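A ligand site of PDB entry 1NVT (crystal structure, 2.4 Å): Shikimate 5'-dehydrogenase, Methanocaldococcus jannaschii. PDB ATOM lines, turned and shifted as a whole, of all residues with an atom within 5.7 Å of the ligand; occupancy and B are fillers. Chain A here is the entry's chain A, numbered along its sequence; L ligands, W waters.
NZ of Lys 162 is in salt-bridge range of O17 of the ligand (2.5 Å).
The side-chain amide nitrogen (ND2) of Asn 157 sits at hydrogen-bond distance from an oxygen (O5) of the ligand, at 2.6 Å.
The guanidinium group (NH2) of Arg 158 is in salt-bridge range of an oxygen (O15) of the ligand (2.7 Å).
N of Leu 256 is in hydrogen-bond range of O14 of the ligand, 2.7 Å away.
The backbone NH of Ala 136 sits at hydrogen-bond distance from an oxygen (O5) of the ligand, at 2.8 Å.
O16 of the ligand lies close to N of Thr 159, at 3.3 Å.
OG1 of Thr 159 sits at hydrogen-bond distance from O16 of the ligand (2.8 Å).
N of Ala 139 lies within hydrogen-bond range of O9 of the ligand (2.8 Å).
A nitrogen (N7) of the ligand is in hydrogen-bond range of the backbone carbonyl oxygen (O) of Leu 229.
A nitrogen (N7) of the ligand lies within hydrogen-bond range of the backbone carbonyl oxygen (O) of Gly 252, at 2.9 Å.
The side-chain sulfur (SD) of Met 205 sits at hydrogen-bond distance from an oxygen (O13) of the ligand.
An oxygen (O12) of the ligand lies within hydrogen-bond range of the backbone carbonyl oxygen (O) of Thr 201 (3.2 Å).
The side-chain amide nitrogen (ND2) of Asn 157 lies close to the backbone NH (N) of Ala 136, at 3.5 Å.
The side-chain amide oxygen of Asn 157 lies within hydrogen-bond range of the side-chain hydroxyl of Thr 159 (3.2 Å).
O of Leu 256 is in hydrogen-bond range of NE2 of Gln 259.
The backbone NH of Leu 229 lies within hydrogen-bond range of the backbone carbonyl oxygen of Asn 199 (3.2 Å).
The backbone NH (N) of Gly 252 lies within hydrogen-bond range of the backbone carbonyl oxygen (O) of Ile 230 (2.9 Å).
The side-chain hydroxyl (OG1) of Thr 201 sits close to the backbone NH (N) of Ile 203 (3.3 Å).
OG1 of Thr 201 lies within hydrogen-bond range of OD1 of Asn 199 (2.7 Å).
O of Tyr 134 is in hydrogen-bond range of N of Ala 200 (2.7 Å).
The backbone nitrogen (N) of Pro 202 lies close to an oxygen (O12) of the ligand (3.5 Å).
The side-chain sulfur (SD) of Met 255 sits close to an oxygen (O14) of the ligand, at 3.5 Å.
Gly 135 touches the ligand (CA to O5, 3.1 Å).
Gly 137 touches the ligand.
Gly 138 touches the ligand.
CD1 of Leu 187 touches C9 of the ligand, 3.8 Å away.
Ala 200 touches the ligand.
Ile 203 touches the ligand.
Ile 230 touches the ligand (CG1 to O12, 3.5 Å).
Tyr 231 touches the ligand.
Hydrophobic or aromatic side chains that line the ligand: Ala 139, Leu 187, Pro 202, Ile 203, Met 205, Ile 230, Tyr 231, Met 255 and Leu 256.
Within 4 Å of the ligand: Gly 135, Ala 136, Gly 137, Gly 138, Ala 139, Asn 157, Arg 158, Thr 159, Lys 162, Leu 187, Ala 200, Thr 201, Pro 202, Ile 203, Met 205, Leu 229, Ile 230, Tyr 231, Gly 252, Met 255 and Leu 256.
The nearest printed residue that does not touch the ligand is Ile 214 (4.8 Å).
Water W2 lies within hydrogen-bond range of the side-chain amide nitrogen of Asn 157 (2.5 Å), the backbone NH of Arg 158 (2.9 Å) and a nitrogen (N5) of the ligand (3.0 Å).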
ATOM      1  N   ASP A 111      -6.426  12.165  17.617  1.00  0.00           N
ATOM      2  CA  ASP A 111      -6.486  11.695  18.987  1.00  0.00           C
ATOM      3  C   ASP A 111      -6.454  12.885  19.945  1.00  0.00           C
ATOM      4  O   ASP A 111      -7.136  12.882  20.973  1.00  0.00           O
ATOM      5  CB  ASP A 111      -5.323  10.741  19.282  1.00  0.00           C
ATOM      6  CG  ASP A 111      -5.417   9.441  18.487  1.00  0.00           C
ATOM      7  OD1 ASP A 111      -6.528   8.872  18.404  1.00  0.00           O
ATOM      8  OD2 ASP A 111      -4.383   8.986  17.960  1.00  0.00           O
ATOM      9  N   TYR A 134      -2.430  11.528  34.009  1.00  0.00           N
ATOM     10  CA  TYR A 134      -1.777  10.338  34.540  1.00  0.00           C
ATOM     11  C   TYR A 134      -1.380   9.455  33.366  1.00  0.00           C
ATOM     12  O   TYR A 134      -2.213   9.095  32.543  1.00  0.00           O
ATOM     13  CB  TYR A 134      -2.719   9.563  35.467  1.00  0.00           C
ATOM     14  CG  TYR A 134      -2.975  10.263  36.780  1.00  0.00           C
ATOM     15  CD1 TYR A 134      -4.179  10.922  37.022  1.00  0.00           C
ATOM     16  CD2 TYR A 134      -1.991  10.285  37.768  1.00  0.00           C
ATOM     17  CE1 TYR A 134      -4.390  11.598  38.223  1.00  0.00           C
ATOM     18  CE2 TYR A 134      -2.190  10.974  38.967  1.00  0.00           C
ATOM     19  CZ  TYR A 134      -3.396  11.623  39.189  1.00  0.00           C
ATOM     20  OH  TYR A 134      -3.596  12.301  40.368  1.00  0.00           O
ATOM     21  N   GLY A 135      -0.103   9.123  33.276  1.00  0.00           N
ATOM     22  CA  GLY A 135       0.373   8.296  32.184  1.00  0.00           C
ATOM     23  C   GLY A 135       1.307   9.085  31.291  1.00  0.00           C
ATOM     24  O   GLY A 135       1.372  10.315  31.396  1.00  0.00           O
ATOM     25  N   ALA A 136       2.005   8.407  30.396  1.00  0.00           N
ATOM     26  CA  ALA A 136       2.928   9.105  29.512  1.00  0.00           C
ATOM     27  C   ALA A 136       3.102   8.390  28.182  1.00  0.00           C
ATOM     28  O   ALA A 136       3.997   8.705  27.404  1.00  0.00           O
ATOM     29  CB  ALA A 136       4.288   9.262  30.206  1.00  0.00           C
ATOM     30  N   GLY A 137       2.230   7.421  27.919  1.00  0.00           N
ATOM     31  CA  GLY A 137       2.300   6.675  26.669  1.00  0.00           C
ATOM     32  C   GLY A 137       1.708   7.458  25.522  1.00  0.00           C
ATOM     33  O   GLY A 137       1.571   8.685  25.583  1.00  0.00           O
ATOM     34  N   GLY A 138       1.331   6.749  24.461  1.00  0.00           N
ATOM     35  CA  GLY A 138       0.741   7.393  23.300  1.00  0.00           C
ATOM     36  C   GLY A 138      -0.503   8.207  23.575  1.00  0.00           C
ATOM     37  O   GLY A 138      -0.688   9.279  22.983  1.00  0.00           O
ATOM     38  N   ALA A 139      -1.378   7.727  24.458  1.00  0.00           N
ATOM     39  CA  ALA A 139      -2.612   8.458  24.761  1.00  0.00           C
ATOM     40  C   ALA A 139      -2.298   9.751  25.506  1.00  0.00           C
ATOM     41  O   ALA A 139      -2.701  10.834  25.077  1.00  0.00           O
ATOM     42  CB  ALA A 139      -3.566   7.596  25.587  1.00  0.00           C
ATOM     43  N   ALA A 140      -1.580   9.646  26.617  1.00  0.00           N
ATOM     44  CA  ALA A 140      -1.220  10.817  27.402  1.00  0.00           C
ATOM     45  C   ALA A 140      -0.458  11.830  26.558  1.00  0.00           C
ATOM     46  O   ALA A 140      -0.566  13.034  26.766  1.00  0.00           O
ATOM     47  CB  ALA A 140      -0.388  10.410  28.602  1.00  0.00           C
ATOM     48  N   ASN A 157       3.542  10.210  36.156  1.00  0.00           N
ATOM     49  CA  ASN A 157       3.748   8.860  35.668  1.00  0.00           C
ATOM     50  C   ASN A 157       4.525   7.967  36.640  1.00  0.00           C
ATOM     51  O   ASN A 157       5.243   8.452  37.518  1.00  0.00           O
ATOM     52  CB  ASN A 157       4.494   8.927  34.333  1.00  0.00           C
ATOM     53  CG  ASN A 157       4.391   7.637  33.545  1.00  0.00           C
ATOM     54  OD1 ASN A 157       5.386   7.107  33.059  1.00  0.00           O
ATOM     55  ND2 ASN A 157       3.166   7.136  33.403  1.00  0.00           N
ATOM     56  N   ARG A 158       4.387   6.653  36.459  1.00  0.00           N
ATOM     57  CA  ARG A 158       5.094   5.695  37.294  1.00  0.00           C
ATOM     58  C   ARG A 158       6.601   5.912  37.121  1.00  0.00           C
ATOM     59  O   ARG A 158       7.337   6.044  38.106  1.00  0.00           O
ATOM     60  CB  ARG A 158       4.707   4.262  36.911  1.00  0.00           C
ATOM     61  CG  ARG A 158       5.560   3.205  37.564  1.00  0.00           C
ATOM     62  CD  ARG A 158       4.998   1.814  37.345  1.00  0.00           C
ATOM     63  NE  ARG A 158       4.716   1.569  35.932  1.00  0.00           N
ATOM     64  CZ  ARG A 158       4.213   0.425  35.463  1.00  0.00           C
ATOM     65  NH1 ARG A 158       3.937  -0.571  36.295  1.00  0.00           N
ATOM     66  NH2 ARG A 158       3.977   0.301  34.165  1.00  0.00           N
ATOM     67  N   THR A 159       7.051   5.943  35.874  1.00  0.00           N
ATOM     68  CA  THR A 159       8.467   6.170  35.602  1.00  0.00           C
ATOM     69  C   THR A 159       8.612   7.672  35.279  1.00  0.00           C
ATOM     70  O   THR A 159       8.338   8.102  34.150  1.00  0.00           O
ATOM     71  CB  THR A 159       8.938   5.312  34.414  1.00  0.00           C
ATOM     72  OG1 THR A 159       8.277   5.720  33.216  1.00  0.00           O
ATOM     73  CG2 THR A 159       8.614   3.841  34.659  1.00  0.00           C
ATOM     74  N   LYS A 162      10.173   9.284  32.094  1.00  0.00           N
ATOM     75  CA  LYS A 162       9.282   9.381  30.940  1.00  0.00           C
ATOM     76  C   LYS A 162       8.434  10.641  31.021  1.00  0.00           C
ATOM     77  O   LYS A 162       8.214  11.323  30.013  1.00  0.00           O
ATOM     78  CB  LYS A 162       8.369   8.145  30.865  1.00  0.00           C
ATOM     79  CG  LYS A 162       8.735   7.170  29.758  1.00  0.00           C
ATOM     80  CD  LYS A 162       7.656   7.121  28.670  1.00  0.00           C
ATOM     81  CE  LYS A 162       6.523   6.175  29.043  1.00  0.00           C
ATOM     82  NZ  LYS A 162       7.022   4.767  29.113  1.00  0.00           N
ATOM     83  N   LEU A 187       3.174   9.636  40.378  1.00  0.00           N
ATOM     84  CA  LEU A 187       1.731   9.445  40.538  1.00  0.00           C
ATOM     85  C   LEU A 187       1.272   9.974  41.887  1.00  0.00           C
ATOM     86  O   LEU A 187       0.082   9.938  42.213  1.00  0.00           O
ATOM     87  CB  LEU A 187       1.402   7.969  40.411  1.00  0.00           C
ATOM     88  CG  LEU A 187       1.780   7.357  39.071  1.00  0.00           C
ATOM     89  CD1 LEU A 187       1.701   5.841  39.143  1.00  0.00           C
ATOM     90  CD2 LEU A 187       0.866   7.897  37.997  1.00  0.00           C
ATOM     91  N   ASN A 199      -7.033  10.118  33.273  1.00  0.00           N
ATOM     92  CA  ASN A 199      -6.303   8.864  33.396  1.00  0.00           C
ATOM     93  C   ASN A 199      -5.970   8.301  32.014  1.00  0.00           C
ATOM     94  O   ASN A 199      -6.848   7.894  31.265  1.00  0.00           O
ATOM     95  CB  ASN A 199      -7.106   7.849  34.199  1.00  0.00           C
ATOM     96  CG  ASN A 199      -6.406   6.515  34.300  1.00  0.00           C
ATOM     97  OD1 ASN A 199      -5.184   6.446  34.320  1.00  0.00           O
ATOM     98  ND2 ASN A 199      -7.185   5.441  34.388  1.00  0.00           N
ATOM     99  N   ALA A 200      -4.681   8.323  31.672  1.00  0.00           N
ATOM    100  CA  ALA A 200      -4.229   7.812  30.385  1.00  0.00           C
ATOM    101  C   ALA A 200      -3.386   6.560  30.604  1.00  0.00           C
ATOM    102  O   ALA A 200      -2.374   6.350  29.930  1.00  0.00           O
ATOM    103  CB  ALA A 200      -3.420   8.875  29.653  1.00  0.00           C
ATOM    104  N   THR A 201      -3.818   5.750  31.569  1.00  0.00           N
ATOM    105  CA  THR A 201      -3.146   4.487  31.904  1.00  0.00           C
ATOM    106  C   THR A 201      -4.184   3.377  31.834  1.00  0.00           C
ATOM    107  O   THR A 201      -5.391   3.638  31.855  1.00  0.00           O
ATOM    108  CB  THR A 201      -2.561   4.490  33.338  1.00  0.00           C
ATOM    109  OG1 THR A 201      -3.606   4.259  34.287  1.00  0.00           O
ATOM    110  CG2 THR A 201      -1.886   5.816  33.643  1.00  0.00           C
ATOM    111  N   PRO A 202      -3.729   2.116  31.760  1.00  0.00           N
ATOM    112  CA  PRO A 202      -4.642   0.961  31.694  1.00  0.00           C
ATOM    113  C   PRO A 202      -5.159   0.471  33.039  1.00  0.00           C
ATOM    114  O   PRO A 202      -5.804  -0.571  33.110  1.00  0.00           O
ATOM    115  CB  PRO A 202      -3.779  -0.114  31.008  1.00  0.00           C
ATOM    116  CG  PRO A 202      -2.702   0.674  30.298  1.00  0.00           C
ATOM    117  CD  PRO A 202      -2.392   1.743  31.302  1.00  0.00           C
ATOM    118  N   ILE A 203      -4.881   1.201  34.107  1.00  0.00           N
ATOM    119  CA  ILE A 203      -5.341   0.772  35.427  1.00  0.00           C
ATOM    120  C   ILE A 203      -6.865   0.746  35.526  1.00  0.00           C
ATOM    121  O   ILE A 203      -7.523   1.775  35.359  1.00  0.00           O
ATOM    122  CB  ILE A 203      -4.768   1.670  36.550  1.00  0.00           C
ATOM    123  CG1 ILE A 203      -3.239   1.568  36.557  1.00  0.00           C
ATOM    124  CG2 ILE A 203      -5.336   1.259  37.899  1.00  0.00           C
ATOM    125  CD1 ILE A 203      -2.577   2.289  37.722  1.00  0.00           C
ATOM    126  N   MET A 205      -8.689  -1.197  33.577  1.00  0.00           N
ATOM    127  CA  MET A 205      -9.148  -1.738  32.298  1.00  0.00           C
ATOM    128  C   MET A 205      -9.200  -3.277  32.344  1.00  0.00           C
ATOM    129  O   MET A 205      -8.355  -3.919  32.972  1.00  0.00           O
ATOM    130  CB  MET A 205      -8.199  -1.285  31.180  1.00  0.00           C
ATOM    131  CG  MET A 205      -8.475  -1.892  29.819  1.00  0.00           C
ATOM    132  SD  MET A 205      -7.281  -1.398  28.565  1.00  0.00           S
ATOM    133  CE  MET A 205      -5.866  -2.381  29.043  1.00  0.00           C
ATOM    134  N   ILE A 214      -6.249   4.777  40.365  1.00  0.00           N
ATOM    135  CA  ILE A 214      -5.017   5.539  40.177  1.00  0.00           C
ATOM    136  C   ILE A 214      -4.897   6.604  41.274  1.00  0.00           C
ATOM    137  O   ILE A 214      -3.825   7.166  41.497  1.00  0.00           O
ATOM    138  CB  ILE A 214      -5.019   6.230  38.787  1.00  0.00           C
ATOM    139  CG1 ILE A 214      -3.638   6.823  38.478  1.00  0.00           C
ATOM    140  CG2 ILE A 214      -6.082   7.315  38.740  1.00  0.00           C
ATOM    141  CD1 ILE A 214      -2.573   5.789  38.180  1.00  0.00           C
ATOM    142  N   LEU A 229      -9.812   7.695  30.088  1.00  0.00           N
ATOM    143  CA  LEU A 229      -9.733   7.277  28.691  1.00  0.00           C
ATOM    144  C   LEU A 229     -10.133   5.808  28.465  1.00  0.00           C
ATOM    145  O   LEU A 229     -10.500   5.415  27.359  1.00  0.00           O
ATOM    146  CB  LEU A 229      -8.326   7.539  28.148  1.00  0.00           C
ATOM    147  CG  LEU A 229      -7.949   9.022  28.050  1.00  0.00           C
ATOM    148  CD1 LEU A 229      -6.537   9.166  27.497  1.00  0.00           C
ATOM    149  CD2 LEU A 229      -8.941   9.730  27.150  1.00  0.00           C
ATOM    150  N   ILE A 230     -10.059   5.007  29.511  1.00  0.00           N
ATOM    151  CA  ILE A 230     -10.429   3.597  29.403  1.00  0.00           C
ATOM    152  C   ILE A 230     -11.901   3.486  28.992  1.00  0.00           C
ATOM    153  O   ILE A 230     -12.701   4.380  29.296  1.00  0.00           O
ATOM    154  CB  ILE A 230     -10.242   2.861  30.751  1.00  0.00           C
ATOM    155  CG1 ILE A 230      -8.765   2.854  31.153  1.00  0.00           C
ATOM    156  CG2 ILE A 230     -10.795   1.441  30.658  1.00  0.00           C
ATOM    157  CD1 ILE A 230      -8.462   2.158  32.475  1.00  0.00           C
ATOM    158  N   TYR A 231     -12.247   2.414  28.290  1.00  0.00           N
ATOM    159  CA  TYR A 231     -13.623   2.177  27.882  1.00  0.00           C
ATOM    160  C   TYR A 231     -14.011   0.700  27.922  1.00  0.00           C
ATOM    161  O   TYR A 231     -14.807   0.231  27.123  1.00  0.00           O
ATOM    162  CB  TYR A 231     -13.911   2.767  26.497  1.00  0.00           C
ATOM    163  CG  TYR A 231     -12.970   2.354  25.378  1.00  0.00           C
ATOM    164  CD1 TYR A 231     -12.852   1.015  24.977  1.00  0.00           C
ATOM    165  CD2 TYR A 231     -12.244   3.311  24.688  1.00  0.00           C
ATOM    166  CE1 TYR A 231     -12.035   0.661  23.903  1.00  0.00           C
ATOM    167  CE2 TYR A 231     -11.425   2.971  23.611  1.00  0.00           C
ATOM    168  CZ  TYR A 231     -11.326   1.642  23.216  1.00  0.00           C
ATOM    169  OH  TYR A 231     -10.534   1.326  22.129  1.00  0.00           O
ATOM    170  N   GLY A 252     -14.250   6.786  28.712  1.00  0.00           N
ATOM    171  CA  GLY A 252     -13.474   6.764  27.477  1.00  0.00           C
ATOM    172  C   GLY A 252     -14.272   6.887  26.201  1.00  0.00           C
ATOM    173  O   GLY A 252     -13.708   7.232  25.150  1.00  0.00           O
ATOM    174  N   LEU A 253     -15.567   6.603  26.270  1.00  0.00           N
ATOM    175  CA  LEU A 253     -16.420   6.677  25.090  1.00  0.00           C
ATOM    176  C   LEU A 253     -16.262   8.015  24.357  1.00  0.00           C
ATOM    177  O   LEU A 253     -16.293   8.064  23.124  1.00  0.00           O
ATOM    178  CB  LEU A 253     -17.883   6.466  25.505  1.00  0.00           C
ATOM    179  CG  LEU A 253     -18.867   6.140  24.388  1.00  0.00           C
ATOM    180  CD1 LEU A 253     -18.421   4.879  23.661  1.00  0.00           C
ATOM    181  CD2 LEU A 253     -20.255   5.941  24.977  1.00  0.00           C
ATOM    182  N   GLY A 254     -16.077   9.080  25.115  1.00  0.00           N
ATOM    183  CA  GLY A 254     -15.928  10.401  24.528  1.00  0.00           C
ATOM    184  C   GLY A 254     -14.772  10.557  23.559  1.00  0.00           C
ATOM    185  O   GLY A 254     -14.960  11.028  22.442  1.00  0.00           O
ATOM    186  N   MET A 255     -13.565  10.175  23.982  1.00  0.00           N
ATOM    187  CA  MET A 255     -12.410  10.314  23.123  1.00  0.00           C
ATOM    188  C   MET A 255     -12.531   9.407  21.892  1.00  0.00           C
ATOM    189  O   MET A 255     -12.329   9.857  20.765  1.00  0.00           O
ATOM    190  CB  MET A 255     -11.112   9.977  23.880  1.00  0.00           C
ATOM    191  CG  MET A 255      -9.828  10.254  23.080  1.00  0.00           C
ATOM    192  SD  MET A 255      -8.304   9.772  23.960  1.00  0.00           S
ATOM    193  CE  MET A 255      -7.067  10.282  22.744  1.00  0.00           C
ATOM    194  N   LEU A 256     -12.879   8.146  22.125  1.00  0.00           N
ATOM    195  CA  LEU A 256     -13.038   7.162  21.059  1.00  0.00           C
ATOM    196  C   LEU A 256     -13.940   7.641  19.929  1.00  0.00           C
ATOM    197  O   LEU A 256     -13.596   7.543  18.743  1.00  0.00           O
ATOM    198  CB  LEU A 256     -13.579   5.845  21.630  1.00  0.00           C
ATOM    199  CG  LEU A 256     -14.148   4.796  20.646  1.00  0.00           C
ATOM    200  CD1 LEU A 256     -13.041   4.323  19.717  1.00  0.00           C
ATOM    201  CD2 LEU A 256     -14.710   3.617  21.424  1.00  0.00           C
ATOM    202  N   ILE A 257     -15.121   8.153  20.301  1.00  0.00           N
ATOM    203  CA  ILE A 257     -16.092   8.629  19.325  1.00  0.00           C
ATOM    204  C   ILE A 257     -15.649   9.900  18.614  1.00  0.00           C
ATOM    205  O   ILE A 257     -15.611   9.940  17.380  1.00  0.00           O
ATOM    206  CB  ILE A 257     -17.453   8.875  19.998  1.00  0.00           C
ATOM    207  CG1 ILE A 257     -18.019   7.530  20.474  1.00  0.00           C
ATOM    208  CG2 ILE A 257     -18.408   9.561  19.037  1.00  0.00           C
ATOM    209  CD1 ILE A 257     -19.191   7.647  21.428  1.00  0.00           C
ATOM    210  N   GLN A 259     -12.695  11.202  18.399  1.00  0.00           N
ATOM    211  CA  GLN A 259     -11.476  10.966  17.636  1.00  0.00           C
ATOM    212  C   GLN A 259     -11.928  10.569  16.225  1.00  0.00           C
ATOM    213  O   GLN A 259     -11.388  11.042  15.226  1.00  0.00           O
ATOM    214  CB  GLN A 259     -10.683   9.829  18.290  1.00  0.00           C
ATOM    215  CG  GLN A 259      -9.601   9.231  17.418  1.00  0.00           C
ATOM    216  CD  GLN A 259     -10.141   8.259  16.392  1.00  0.00           C
ATOM    217  OE1 GLN A 259      -9.888   8.394  15.192  1.00  0.00           O
ATOM    218  NE2 GLN A 259     -10.906   7.261  16.854  1.00  0.00           N
HETATM  219  P1  LIG L   1       0.536   2.835  26.721  1.00  0.00           P
HETATM  220  O1  LIG L   1       1.691   2.415  25.846  1.00  0.00           O
HETATM  221  O2  LIG L   1      -0.321   1.662  27.186  1.00  0.00           O
HETATM  222  O3  LIG L   1       1.037   3.645  27.911  1.00  0.00           O
HETATM  223  C1  LIG L   1       1.488   3.015  29.096  1.00  0.00           C
HETATM  224  C2  LIG L   1       1.217   3.849  30.331  1.00  0.00           C
HETATM  225  O4  LIG L   1       0.748   2.969  31.366  1.00  0.00           O
HETATM  226  C3  LIG L   1       2.452   4.540  30.928  1.00  0.00           C
HETATM  227  O5  LIG L   1       2.150   5.850  31.405  1.00  0.00           O
HETATM  228  C4  LIG L   1       2.889   3.574  32.032  1.00  0.00           C
HETATM  229  O6  LIG L   1       3.708   4.193  33.100  1.00  0.00           O
HETATM  230  C5  LIG L   1       1.543   3.158  32.519  1.00  0.00           C
HETATM  231  N1  LIG L   1       1.107   2.164  33.378  1.00  0.00           N
HETATM  232  C6  LIG L   1       0.868   0.881  32.915  1.00  0.00           C
HETATM  233  N2  LIG L   1       0.635   0.035  33.944  1.00  0.00           N
HETATM  234  C7  LIG L   1       0.709   0.826  35.052  1.00  0.00           C
HETATM  235  C8  LIG L   1       0.549   0.450  36.395  1.00  0.00           C
HETATM  236  N3  LIG L   1       0.286  -0.795  36.744  1.00  0.00           N
HETATM  237  N4  LIG L   1       0.676   1.426  37.392  1.00  0.00           N
HETATM  238  C9  LIG L   1       0.958   2.735  37.054  1.00  0.00           C
HETATM  239  N5  LIG L   1       1.114   3.080  35.737  1.00  0.00           N
HETATM  240  C10 LIG L   1       0.991   2.138  34.727  1.00  0.00           C
HETATM  241  O7  LIG L   1      -0.413   3.780  26.054  1.00  0.00           O
HETATM  242  P2  LIG L   1      -1.874   3.812  25.769  1.00  0.00           P
HETATM  243  O8  LIG L   1      -2.114   2.656  24.819  1.00  0.00           O
HETATM  244  O9  LIG L   1      -2.184   5.107  25.080  1.00  0.00           O
HETATM  245  O10 LIG L   1      -2.762   3.672  26.991  1.00  0.00           O
HETATM  246  C11 LIG L   1      -3.790   4.226  27.810  1.00  0.00           C
HETATM  247  C12 LIG L   1      -5.264   3.949  27.956  1.00  0.00           C
HETATM  248  O11 LIG L   1      -5.973   4.525  26.861  1.00  0.00           O
HETATM  249  C13 LIG L   1      -5.473   2.457  27.950  1.00  0.00           C
HETATM  250  O12 LIG L   1      -6.044   1.953  29.171  1.00  0.00           O
HETATM  251  C14 LIG L   1      -6.320   2.182  26.719  1.00  0.00           C
HETATM  252  O13 LIG L   1      -7.502   1.479  27.126  1.00  0.00           O
HETATM  253  C15 LIG L   1      -6.635   3.509  26.090  1.00  0.00           C
HETATM  254  N6  LIG L   1      -7.175   4.366  25.158  1.00  0.00           N
HETATM  255  C16 LIG L   1      -8.471   4.977  25.002  1.00  0.00           C
HETATM  256  C17 LIG L   1      -8.724   5.815  23.870  1.00  0.00           C
HETATM  257  C18 LIG L   1     -10.086   6.463  23.674  1.00  0.00           C
HETATM  258  O14 LIG L   1     -10.309   7.298  22.541  1.00  0.00           O
HETATM  259  N7  LIG L   1     -11.013   6.203  24.623  1.00  0.00           N
HETATM  260  C19 LIG L   1      -7.689   6.057  22.891  1.00  0.00           C
HETATM  261  C20 LIG L   1      -6.312   5.451  23.008  1.00  0.00           C
HETATM  262  C21 LIG L   1      -6.095   4.564  24.214  1.00  0.00           C
HETATM  263  P3  LIG L   1       4.953   3.596  32.352  1.00  0.00           P
HETATM  264  O15 LIG L   1       4.827   2.047  32.287  1.00  0.00           O
HETATM  265  O16 LIG L   1       6.027   4.092  33.302  1.00  0.00           O
HETATM  266  O17 LIG L   1       5.484   4.034  31.007  1.00  0.00           O
HETATM  267  O   HOH W   1       3.547   0.428  25.104  1.00  0.00           O
HETATM  268  O   HOH W   2       1.866   5.906  35.184  1.00  0.00           O
HETATM  269  O   HOH W   3      -4.107   1.350  23.790  1.00  0.00           O
